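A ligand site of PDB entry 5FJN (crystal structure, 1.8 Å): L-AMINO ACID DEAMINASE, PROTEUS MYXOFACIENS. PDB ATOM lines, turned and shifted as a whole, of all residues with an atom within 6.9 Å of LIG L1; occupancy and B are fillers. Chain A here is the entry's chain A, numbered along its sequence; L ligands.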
ATOM      1  N   TYR A  80      10.910   3.587 -12.486  1.00  0.00           N
ATOM      2  CA  TYR A  80      11.031   2.181 -12.125  1.00  0.00           C
ATOM      3  C   TYR A  80      10.042   1.890 -11.013  1.00  0.00           C
ATOM      4  O   TYR A  80       9.381   0.859 -11.008  1.00  0.00           O
ATOM      5  CB  TYR A  80      12.454   1.894 -11.654  1.00  0.00           C
ATOM      6  CG  TYR A  80      12.709   0.474 -11.221  1.00  0.00           C
ATOM      7  CD1 TYR A  80      12.261  -0.610 -11.976  1.00  0.00           C
ATOM      8  CD2 TYR A  80      13.437   0.203 -10.062  1.00  0.00           C
ATOM      9  CE1 TYR A  80      12.514  -1.911 -11.581  1.00  0.00           C
ATOM     10  CE2 TYR A  80      13.683  -1.087  -9.663  1.00  0.00           C
ATOM     11  CZ  TYR A  80      13.227  -2.140 -10.425  1.00  0.00           C
ATOM     12  OH  TYR A  80      13.488  -3.421 -10.024  1.00  0.00           O
ATOM     13  N   SER A  81       9.982   2.815 -10.061  1.00  0.00           N
ATOM     14  CA  SER A  81       8.865   2.951  -9.132  1.00  0.00           C
ATOM     15  C   SER A  81       8.835   1.907  -8.001  1.00  0.00           C
ATOM     16  O   SER A  81       7.780   1.399  -7.625  1.00  0.00           O
ATOM     17  CB  SER A  81       7.543   2.962  -9.911  1.00  0.00           C
ATOM     18  OG  SER A  81       6.562   3.715  -9.226  1.00  0.00           O
ATOM     19  N   GLN A  82      10.018   1.609  -7.468  1.00  0.00           N
ATOM     20  CA  GLN A  82      10.119   0.856  -6.227  1.00  0.00           C
ATOM     21  C   GLN A  82       9.978   1.808  -5.041  1.00  0.00           C
ATOM     22  O   GLN A  82      10.610   2.882  -4.994  1.00  0.00           O
ATOM     23  CB  GLN A  82      11.415   0.031  -6.153  1.00  0.00           C
ATOM     24  CG  GLN A  82      12.716   0.818  -6.138  1.00  0.00           C
ATOM     25  CD  GLN A  82      13.938  -0.078  -6.157  1.00  0.00           C
ATOM     26  OE1 GLN A  82      13.891  -1.239  -5.725  1.00  0.00           O
ATOM     27  NE2 GLN A  82      15.058   0.452  -6.654  1.00  0.00           N
ATOM     28  N   ILE A  84      10.641   2.292  -1.401  1.00  0.00           N
ATOM     29  CA  ILE A  84      11.550   1.694  -0.433  1.00  0.00           C
ATOM     30  C   ILE A  84      12.207   2.705   0.502  1.00  0.00           C
ATOM     31  O   ILE A  84      12.286   3.898   0.190  1.00  0.00           O
ATOM     32  CB  ILE A  84      12.677   0.892  -1.134  1.00  0.00           C
ATOM     33  CG1 ILE A  84      13.600   1.802  -1.947  1.00  0.00           C
ATOM     34  CG2 ILE A  84      12.095  -0.170  -2.043  1.00  0.00           C
ATOM     35  CD1 ILE A  84      14.873   1.120  -2.414  1.00  0.00           C
ATOM     36  N   ARG A 121      11.187  -6.656  -0.973  1.00  0.00           N
ATOM     37  CA  ARG A 121      12.348  -6.474  -1.847  1.00  0.00           C
ATOM     38  C   ARG A 121      13.547  -7.247  -1.317  1.00  0.00           C
ATOM     39  O   ARG A 121      13.997  -6.993  -0.195  1.00  0.00           O
ATOM     40  CB  ARG A 121      12.716  -4.991  -1.922  1.00  0.00           C
ATOM     41  CG  ARG A 121      13.957  -4.672  -2.744  1.00  0.00           C
ATOM     42  CD  ARG A 121      14.168  -3.165  -2.772  1.00  0.00           C
ATOM     43  NE  ARG A 121      15.250  -2.768  -3.675  1.00  0.00           N
ATOM     44  CZ  ARG A 121      16.531  -2.640  -3.344  1.00  0.00           C
ATOM     45  NH1 ARG A 121      16.955  -2.877  -2.108  1.00  0.00           N
ATOM     46  NH2 ARG A 121      17.404  -2.250  -4.273  1.00  0.00           N
ATOM     47  N   LEU A 261      17.935   8.114 -18.327  1.00  0.00           N
ATOM     48  CA  LEU A 261      17.701   6.737 -17.914  1.00  0.00           C
ATOM     49  C   LEU A 261      16.874   5.997 -18.955  1.00  0.00           C
ATOM     50  O   LEU A 261      16.178   6.631 -19.761  1.00  0.00           O
ATOM     51  CB  LEU A 261      16.941   6.743 -16.589  1.00  0.00           C
ATOM     52  CG  LEU A 261      17.725   7.325 -15.411  1.00  0.00           C
ATOM     53  CD1 LEU A 261      16.803   7.868 -14.334  1.00  0.00           C
ATOM     54  CD2 LEU A 261      18.661   6.277 -14.842  1.00  0.00           C
ATOM     55  N   GLN A 263      14.161   2.437 -19.316  1.00  0.00           N
ATOM     56  CA  GLN A 263      13.340   1.489 -18.575  1.00  0.00           C
ATOM     57  C   GLN A 263      12.599   0.571 -19.533  1.00  0.00           C
ATOM     58  O   GLN A 263      12.421   0.886 -20.711  1.00  0.00           O
ATOM     59  CB  GLN A 263      12.300   2.235 -17.725  1.00  0.00           C
ATOM     60  CG  GLN A 263      12.888   3.024 -16.566  1.00  0.00           C
ATOM     61  CD  GLN A 263      13.443   2.139 -15.467  1.00  0.00           C
ATOM     62  OE1 GLN A 263      12.934   1.057 -15.203  1.00  0.00           O
ATOM     63  NE2 GLN A 263      14.503   2.608 -14.815  1.00  0.00           N
ATOM     64  N   HIS A 284      17.946  -6.087 -11.882  1.00  0.00           N
ATOM     65  CA  HIS A 284      16.978  -5.387 -11.052  1.00  0.00           C
ATOM     66  C   HIS A 284      15.616  -5.466 -11.721  1.00  0.00           C
ATOM     67  O   HIS A 284      15.431  -4.944 -12.820  1.00  0.00           O
ATOM     68  CB  HIS A 284      17.393  -3.915 -10.863  1.00  0.00           C
ATOM     69  CG  HIS A 284      18.862  -3.678 -10.966  1.00  0.00           C
ATOM     70  ND1 HIS A 284      19.481  -3.298 -12.137  1.00  0.00           N
ATOM     71  CD2 HIS A 284      19.847  -3.761 -10.039  1.00  0.00           C
ATOM     72  CE1 HIS A 284      20.774  -3.160 -11.931  1.00  0.00           C
ATOM     73  NE2 HIS A 284      21.023  -3.444 -10.668  1.00  0.00           N
ATOM     74  N   ALA A 296      15.026  -2.609 -14.786  1.00  0.00           N
ATOM     75  CA  ALA A 296      15.826  -1.398 -14.798  1.00  0.00           C
ATOM     76  C   ALA A 296      17.296  -1.730 -15.009  1.00  0.00           C
ATOM     77  O   ALA A 296      17.848  -2.545 -14.286  1.00  0.00           O
ATOM     78  CB  ALA A 296      15.664  -0.658 -13.474  1.00  0.00           C
ATOM     79  N   PRO A 297      17.929  -1.127 -16.034  1.00  0.00           N
ATOM     80  CA  PRO A 297      19.386  -1.218 -16.153  1.00  0.00           C
ATOM     81  C   PRO A 297      20.124  -0.557 -14.986  1.00  0.00           C
ATOM     82  O   PRO A 297      21.211  -0.994 -14.611  1.00  0.00           O
ATOM     83  CB  PRO A 297      19.687  -0.463 -17.461  1.00  0.00           C
ATOM     84  CG  PRO A 297      18.424  -0.504 -18.239  1.00  0.00           C
ATOM     85  CD  PRO A 297      17.302  -0.520 -17.231  1.00  0.00           C
ATOM     86  N   ARG A 298      19.527   0.490 -14.427  1.00  0.00           N
ATOM     87  CA  ARG A 298      20.144   1.301 -13.367  1.00  0.00           C
ATOM     88  C   ARG A 298      21.530   1.793 -13.802  1.00  0.00           C
ATOM     89  O   ARG A 298      22.501   1.719 -13.043  1.00  0.00           O
ATOM     90  CB  ARG A 298      20.199   0.537 -12.040  1.00  0.00           C
ATOM     91  CG  ARG A 298      18.839   0.024 -11.573  1.00  0.00           C
ATOM     92  CD  ARG A 298      18.862  -0.482 -10.130  1.00  0.00           C
ATOM     93  NE  ARG A 298      18.347   0.496  -9.163  1.00  0.00           N
ATOM     94  CZ  ARG A 298      19.025   0.976  -8.117  1.00  0.00           C
ATOM     95  NH1 ARG A 298      20.272   0.606  -7.865  1.00  0.00           N
ATOM     96  NH2 ARG A 298      18.435   1.852  -7.310  1.00  0.00           N
ATOM     97  N   ILE A 299      21.612   2.279 -15.039  1.00  0.00           N
ATOM     98  CA  ILE A 299      22.806   2.926 -15.563  1.00  0.00           C
ATOM     99  C   ILE A 299      22.442   4.367 -15.907  1.00  0.00           C
ATOM    100  O   ILE A 299      21.391   4.613 -16.496  1.00  0.00           O
ATOM    101  CB  ILE A 299      23.368   2.227 -16.814  1.00  0.00           C
ATOM    102  CG1 ILE A 299      23.670   0.752 -16.501  1.00  0.00           C
ATOM    103  CG2 ILE A 299      24.628   2.940 -17.298  1.00  0.00           C
ATOM    104  CD1 ILE A 299      23.930  -0.105 -17.728  1.00  0.00           C
ATOM    105  N   PHE A 300      23.314   5.291 -15.532  1.00  0.00           N
ATOM    106  CA  PHE A 300      23.063   6.717 -15.699  1.00  0.00           C
ATOM    107  C   PHE A 300      23.846   7.251 -16.882  1.00  0.00           C
ATOM    108  O   PHE A 300      25.013   6.925 -17.063  1.00  0.00           O
ATOM    109  CB  PHE A 300      23.462   7.474 -14.423  1.00  0.00           C
ATOM    110  CG  PHE A 300      22.771   6.996 -13.169  1.00  0.00           C
ATOM    111  CD1 PHE A 300      21.556   6.321 -13.229  1.00  0.00           C
ATOM    112  CD2 PHE A 300      23.324   7.241 -11.910  1.00  0.00           C
ATOM    113  CE1 PHE A 300      20.919   5.892 -12.067  1.00  0.00           C
ATOM    114  CE2 PHE A 300      22.691   6.820 -10.764  1.00  0.00           C
ATOM    115  CZ  PHE A 300      21.480   6.142 -10.837  1.00  0.00           C
ATOM    116  N   VAL A 394      15.872  12.464 -15.195  1.00  0.00           N
ATOM    117  CA  VAL A 394      15.765  12.938 -13.802  1.00  0.00           C
ATOM    118  C   VAL A 394      16.709  14.119 -13.619  1.00  0.00           C
ATOM    119  O   VAL A 394      17.589  14.345 -14.464  1.00  0.00           O
ATOM    120  CB  VAL A 394      16.090  11.862 -12.744  1.00  0.00           C
ATOM    121  CG1 VAL A 394      14.956  10.879 -12.631  1.00  0.00           C
ATOM    122  CG2 VAL A 394      17.394  11.137 -13.040  1.00  0.00           C
ATOM    123  N   THR A 419      14.148  15.554  -6.738  1.00  0.00           N
ATOM    124  CA  THR A 419      14.322  14.261  -6.097  1.00  0.00           C
ATOM    125  C   THR A 419      14.369  13.142  -7.127  1.00  0.00           C
ATOM    126  O   THR A 419      13.689  13.208  -8.156  1.00  0.00           O
ATOM    127  CB  THR A 419      13.224  13.969  -5.047  1.00  0.00           C
ATOM    128  OG1 THR A 419      13.470  12.700  -4.438  1.00  0.00           O
ATOM    129  CG2 THR A 419      11.822  13.977  -5.660  1.00  0.00           C
ATOM    130  N   VAL A 420      15.153  12.110  -6.840  1.00  0.00           N
ATOM    131  CA  VAL A 420      15.160  10.889  -7.632  1.00  0.00           C
ATOM    132  C   VAL A 420      14.435   9.756  -6.908  1.00  0.00           C
ATOM    133  O   VAL A 420      14.506   8.598  -7.320  1.00  0.00           O
ATOM    134  CB  VAL A 420      16.587  10.482  -8.061  1.00  0.00           C
ATOM    135  CG1 VAL A 420      17.178  11.564  -8.948  1.00  0.00           C
ATOM    136  CG2 VAL A 420      17.484  10.198  -6.852  1.00  0.00           C
ATOM    137  N   TRP A 421      13.713  10.100  -5.828  1.00  0.00           N
ATOM    138  CA  TRP A 421      12.928   9.138  -5.061  1.00  0.00           C
ATOM    139  C   TRP A 421      11.502   9.671  -4.824  1.00  0.00           C
ATOM    140  O   TRP A 421      10.874   9.386  -3.791  1.00  0.00           O
ATOM    141  CB  TRP A 421      13.618   8.826  -3.725  1.00  0.00           C
ATOM    142  CG  TRP A 421      14.822   7.947  -3.862  1.00  0.00           C
ATOM    143  CD1 TRP A 421      16.129   8.338  -3.743  1.00  0.00           C
ATOM    144  CD2 TRP A 421      14.851   6.546  -4.158  1.00  0.00           C
ATOM    145  NE1 TRP A 421      16.964   7.260  -3.931  1.00  0.00           N
ATOM    146  CE2 TRP A 421      16.207   6.157  -4.194  1.00  0.00           C
ATOM    147  CE3 TRP A 421      13.862   5.581  -4.391  1.00  0.00           C
ATOM    148  CZ2 TRP A 421      16.592   4.842  -4.451  1.00  0.00           C
ATOM    149  CZ3 TRP A 421      14.250   4.286  -4.651  1.00  0.00           C
ATOM    150  CH2 TRP A 421      15.607   3.918  -4.676  1.00  0.00           C
ATOM    151  N   GLY A 422      10.999  10.421  -5.797  1.00  0.00           N
ATOM    152  CA  GLY A 422       9.709  11.089  -5.671  1.00  0.00           C
ATOM    153  C   GLY A 422       8.475  10.191  -5.664  1.00  0.00           C
ATOM    154  O   GLY A 422       7.439  10.583  -5.133  1.00  0.00           O
HETATM  155  C1  LIG L   1      15.972   3.068  -9.253  1.00  0.00           C
HETATM  156  O1  LIG L   1      15.514   2.893  -8.104  1.00  0.00           O
HETATM  157  O2  LIG L   1      16.275   2.098  -9.999  1.00  0.00           O
HETATM  158  C2  LIG L   1      16.182   4.467  -9.757  1.00  0.00           C
HETATM  159  C3  LIG L   1      15.769   5.659  -8.952  1.00  0.00           C
HETATM  160  C4  LIG L   1      15.988   6.920  -9.480  1.00  0.00           C
HETATM  161  N1  LIG L   1      15.188   5.537  -7.731  1.00  0.00           N
HETATM  162  C5  LIG L   1      16.574   7.079 -10.729  1.00  0.00           C
HETATM  163  C6  LIG L   1      16.961   5.971 -11.474  1.00  0.00           C
HETATM  164  C7  LIG L   1      16.759   4.679 -11.003  1.00  0.00           C
HETATM  165  P1  LG2 L   2       7.431  15.152 -12.739  1.00  0.00           P
HETATM  166  O1  LG2 L   2       8.500  15.329 -13.766  1.00  0.00           O
HETATM  167  O2  LG2 L   2       6.728  13.822 -12.652  1.00  0.00           O
HETATM  168  O3  LG2 L   2       6.328  16.295 -12.929  1.00  0.00           O
HETATM  169  C1  LG2 L   2       6.647  17.642 -13.228  1.00  0.00           C
HETATM  170  C2  LG2 L   2       5.568  18.107 -14.182  1.00  0.00           C
HETATM  171  O4  LG2 L   2       5.566  19.521 -14.265  1.00  0.00           O
HETATM  172  C3  LG2 L   2       5.754  17.546 -15.584  1.00  0.00           C
HETATM  173  O5  LG2 L   2       4.604  16.758 -15.925  1.00  0.00           O
HETATM  174  C4  LG2 L   2       5.933  18.786 -16.450  1.00  0.00           C
HETATM  175  O6  LG2 L   2       5.323  18.659 -17.737  1.00  0.00           O
HETATM  176  C5  LG2 L   2       5.285  19.881 -15.616  1.00  0.00           C
HETATM  177  N1  LG2 L   2       5.823  21.238 -15.791  1.00  0.00           N
HETATM  178  C6  LG2 L   2       7.113  21.610 -15.673  1.00  0.00           C
HETATM  179  N2  LG2 L   2       7.230  22.937 -15.860  1.00  0.00           N
HETATM  180  C7  LG2 L   2       6.001  23.441 -16.081  1.00  0.00           C
HETATM  181  C8  LG2 L   2       5.413  24.766 -16.368  1.00  0.00           C
HETATM  182  N3  LG2 L   2       6.205  25.856 -16.442  1.00  0.00           N
HETATM  183  N4  LG2 L   2       4.083  24.855 -16.537  1.00  0.00           N
HETATM  184  C9  LG2 L   2       3.270  23.769 -16.462  1.00  0.00           C
HETATM  185  N5  LG2 L   2       3.748  22.529 -16.217  1.00  0.00           N
HETATM  186  C10 LG2 L   2       5.069  22.312 -16.027  1.00  0.00           C
HETATM  187  N6  LG2 L   2      11.359   7.213  -7.424  1.00  0.00           N
HETATM  188  C11 LG2 L   2      11.192   6.271  -6.470  1.00  0.00           C
HETATM  189  O7  LG2 L   2      10.765   6.640  -5.347  1.00  0.00           O
HETATM  190  N7  LG2 L   2      11.455   4.974  -6.678  1.00  0.00           N
HETATM  191  C12 LG2 L   2      11.903   4.520  -7.869  1.00  0.00           C
HETATM  192  O8  LG2 L   2      12.144   3.320  -8.078  1.00  0.00           O
HETATM  193  C13 LG2 L   2      12.115   5.476  -8.955  1.00  0.00           C
HETATM  194  N8  LG2 L   2      12.573   5.088 -10.178  1.00  0.00           N
HETATM  195  C14 LG2 L   2      12.759   5.991 -11.164  1.00  0.00           C
HETATM  196  C15 LG2 L   2      13.221   5.566 -12.423  1.00  0.00           C
HETATM  197  C16 LG2 L   2      13.396   6.475 -13.450  1.00  0.00           C
HETATM  198  C17 LG2 L   2      13.887   5.991 -14.795  1.00  0.00           C
HETATM  199  C18 LG2 L   2      13.105   7.905 -13.207  1.00  0.00           C
HETATM  200  C19 LG2 L   2      13.278   8.906 -14.317  1.00  0.00           C
HETATM  201  C20 LG2 L   2      12.644   8.347 -11.973  1.00  0.00           C
HETATM  202  C21 LG2 L   2      12.455   7.433 -10.926  1.00  0.00           C
HETATM  203  N9  LG2 L   2      11.987   7.841  -9.650  1.00  0.00           N
HETATM  204  C22 LG2 L   2      11.814   6.885  -8.658  1.00  0.00           C
HETATM  205  C23 LG2 L   2      11.737   9.237  -9.302  1.00  0.00           C
HETATM  206  C24 LG2 L   2      10.365   9.778  -9.519  1.00  0.00           C
HETATM  207  O9  LG2 L   2       9.883   9.275 -10.766  1.00  0.00           O
HETATM  208  C25 LG2 L   2      10.507  11.293  -9.507  1.00  0.00           C
HETATM  209  O10 LG2 L   2      11.313  11.749  -8.397  1.00  0.00           O
HETATM  210  C26 LG2 L   2       9.138  11.901  -9.389  1.00  0.00           C
HETATM  211  O11 LG2 L   2       8.339  11.397 -10.466  1.00  0.00           O
HETATM  212  C27 LG2 L   2       9.247  13.404  -9.426  1.00  0.00           C
HETATM  213  O12 LG2 L   2       7.926  13.911  -9.462  1.00  0.00           O
HETATM  214  P2  LG2 L   2       7.651  15.425  -9.829  1.00  0.00           P
HETATM  215  O13 LG2 L   2       6.173  15.644  -9.701  1.00  0.00           O
HETATM  216  O14 LG2 L   2       8.593  16.268  -9.001  1.00  0.00           O
HETATM  217  O15 LG2 L   2       8.161  15.568 -11.359  1.00  0.00           O
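CD2 of Tyr 80 touches O2 of LIG L1 (3.4 Å).
Leu 261 touches LIG L1 (CD1 to C6, 3.4 Å).
Trp 421 touches LIG L1.
Hydrophobic or aromatic side chains that line LIG L1: Tyr 80, Leu 261, Val 420 and Trp 421.
The nearest printed residue that does not touch LIG L1 is Phe 300 (4.003 Å).
The side-chain amide oxygen (OE1) of Gln 82 lies within hydrogen-bond range of the guanidinium group (NE) of Arg 121 (2.9 Å).
The backbone NH (N) of Trp 421 lies within hydrogen-bond range of the side-chain hydroxyl (OG1) of Thr 419 (3.0 Å).
O of Val 420 lies close to N1 of LIG L1.
The side-chain amide nitrogen of Gln 82 is in hydrogen-bond range of an oxygen (O1) of LIG L1.
An oxygen (O8) of LG2 L2 lies within hydrogen-bond range of the backbone NH of Gln 82.
The backbone NH (N) of Tyr 80 sits close to a nitrogen (N8) of LG2 L2, 3.2 Å away.
The backbone carbonyl oxygen (O) of Gln 82 lies within hydrogen-bond range of a nitrogen (N7) of LG2 L2, at 2.8 Å.
An oxygen (O10) of LG2 L2 lies within hydrogen-bond range of the backbone NH (N) of Gly 422.
The backbone carbonyl oxygen of Thr 419 is in hydrogen-bond range of an oxygen (O10) of LG2 L2, 2.8 Å away.
The backbone NH of Ser 81 is in hydrogen-bond range of an oxygen (O8) of LG2 L2, at 3.0 Å.
O2 of LIG L1 lies within salt-bridge range of NE of Arg 298, at 2.7 Å.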
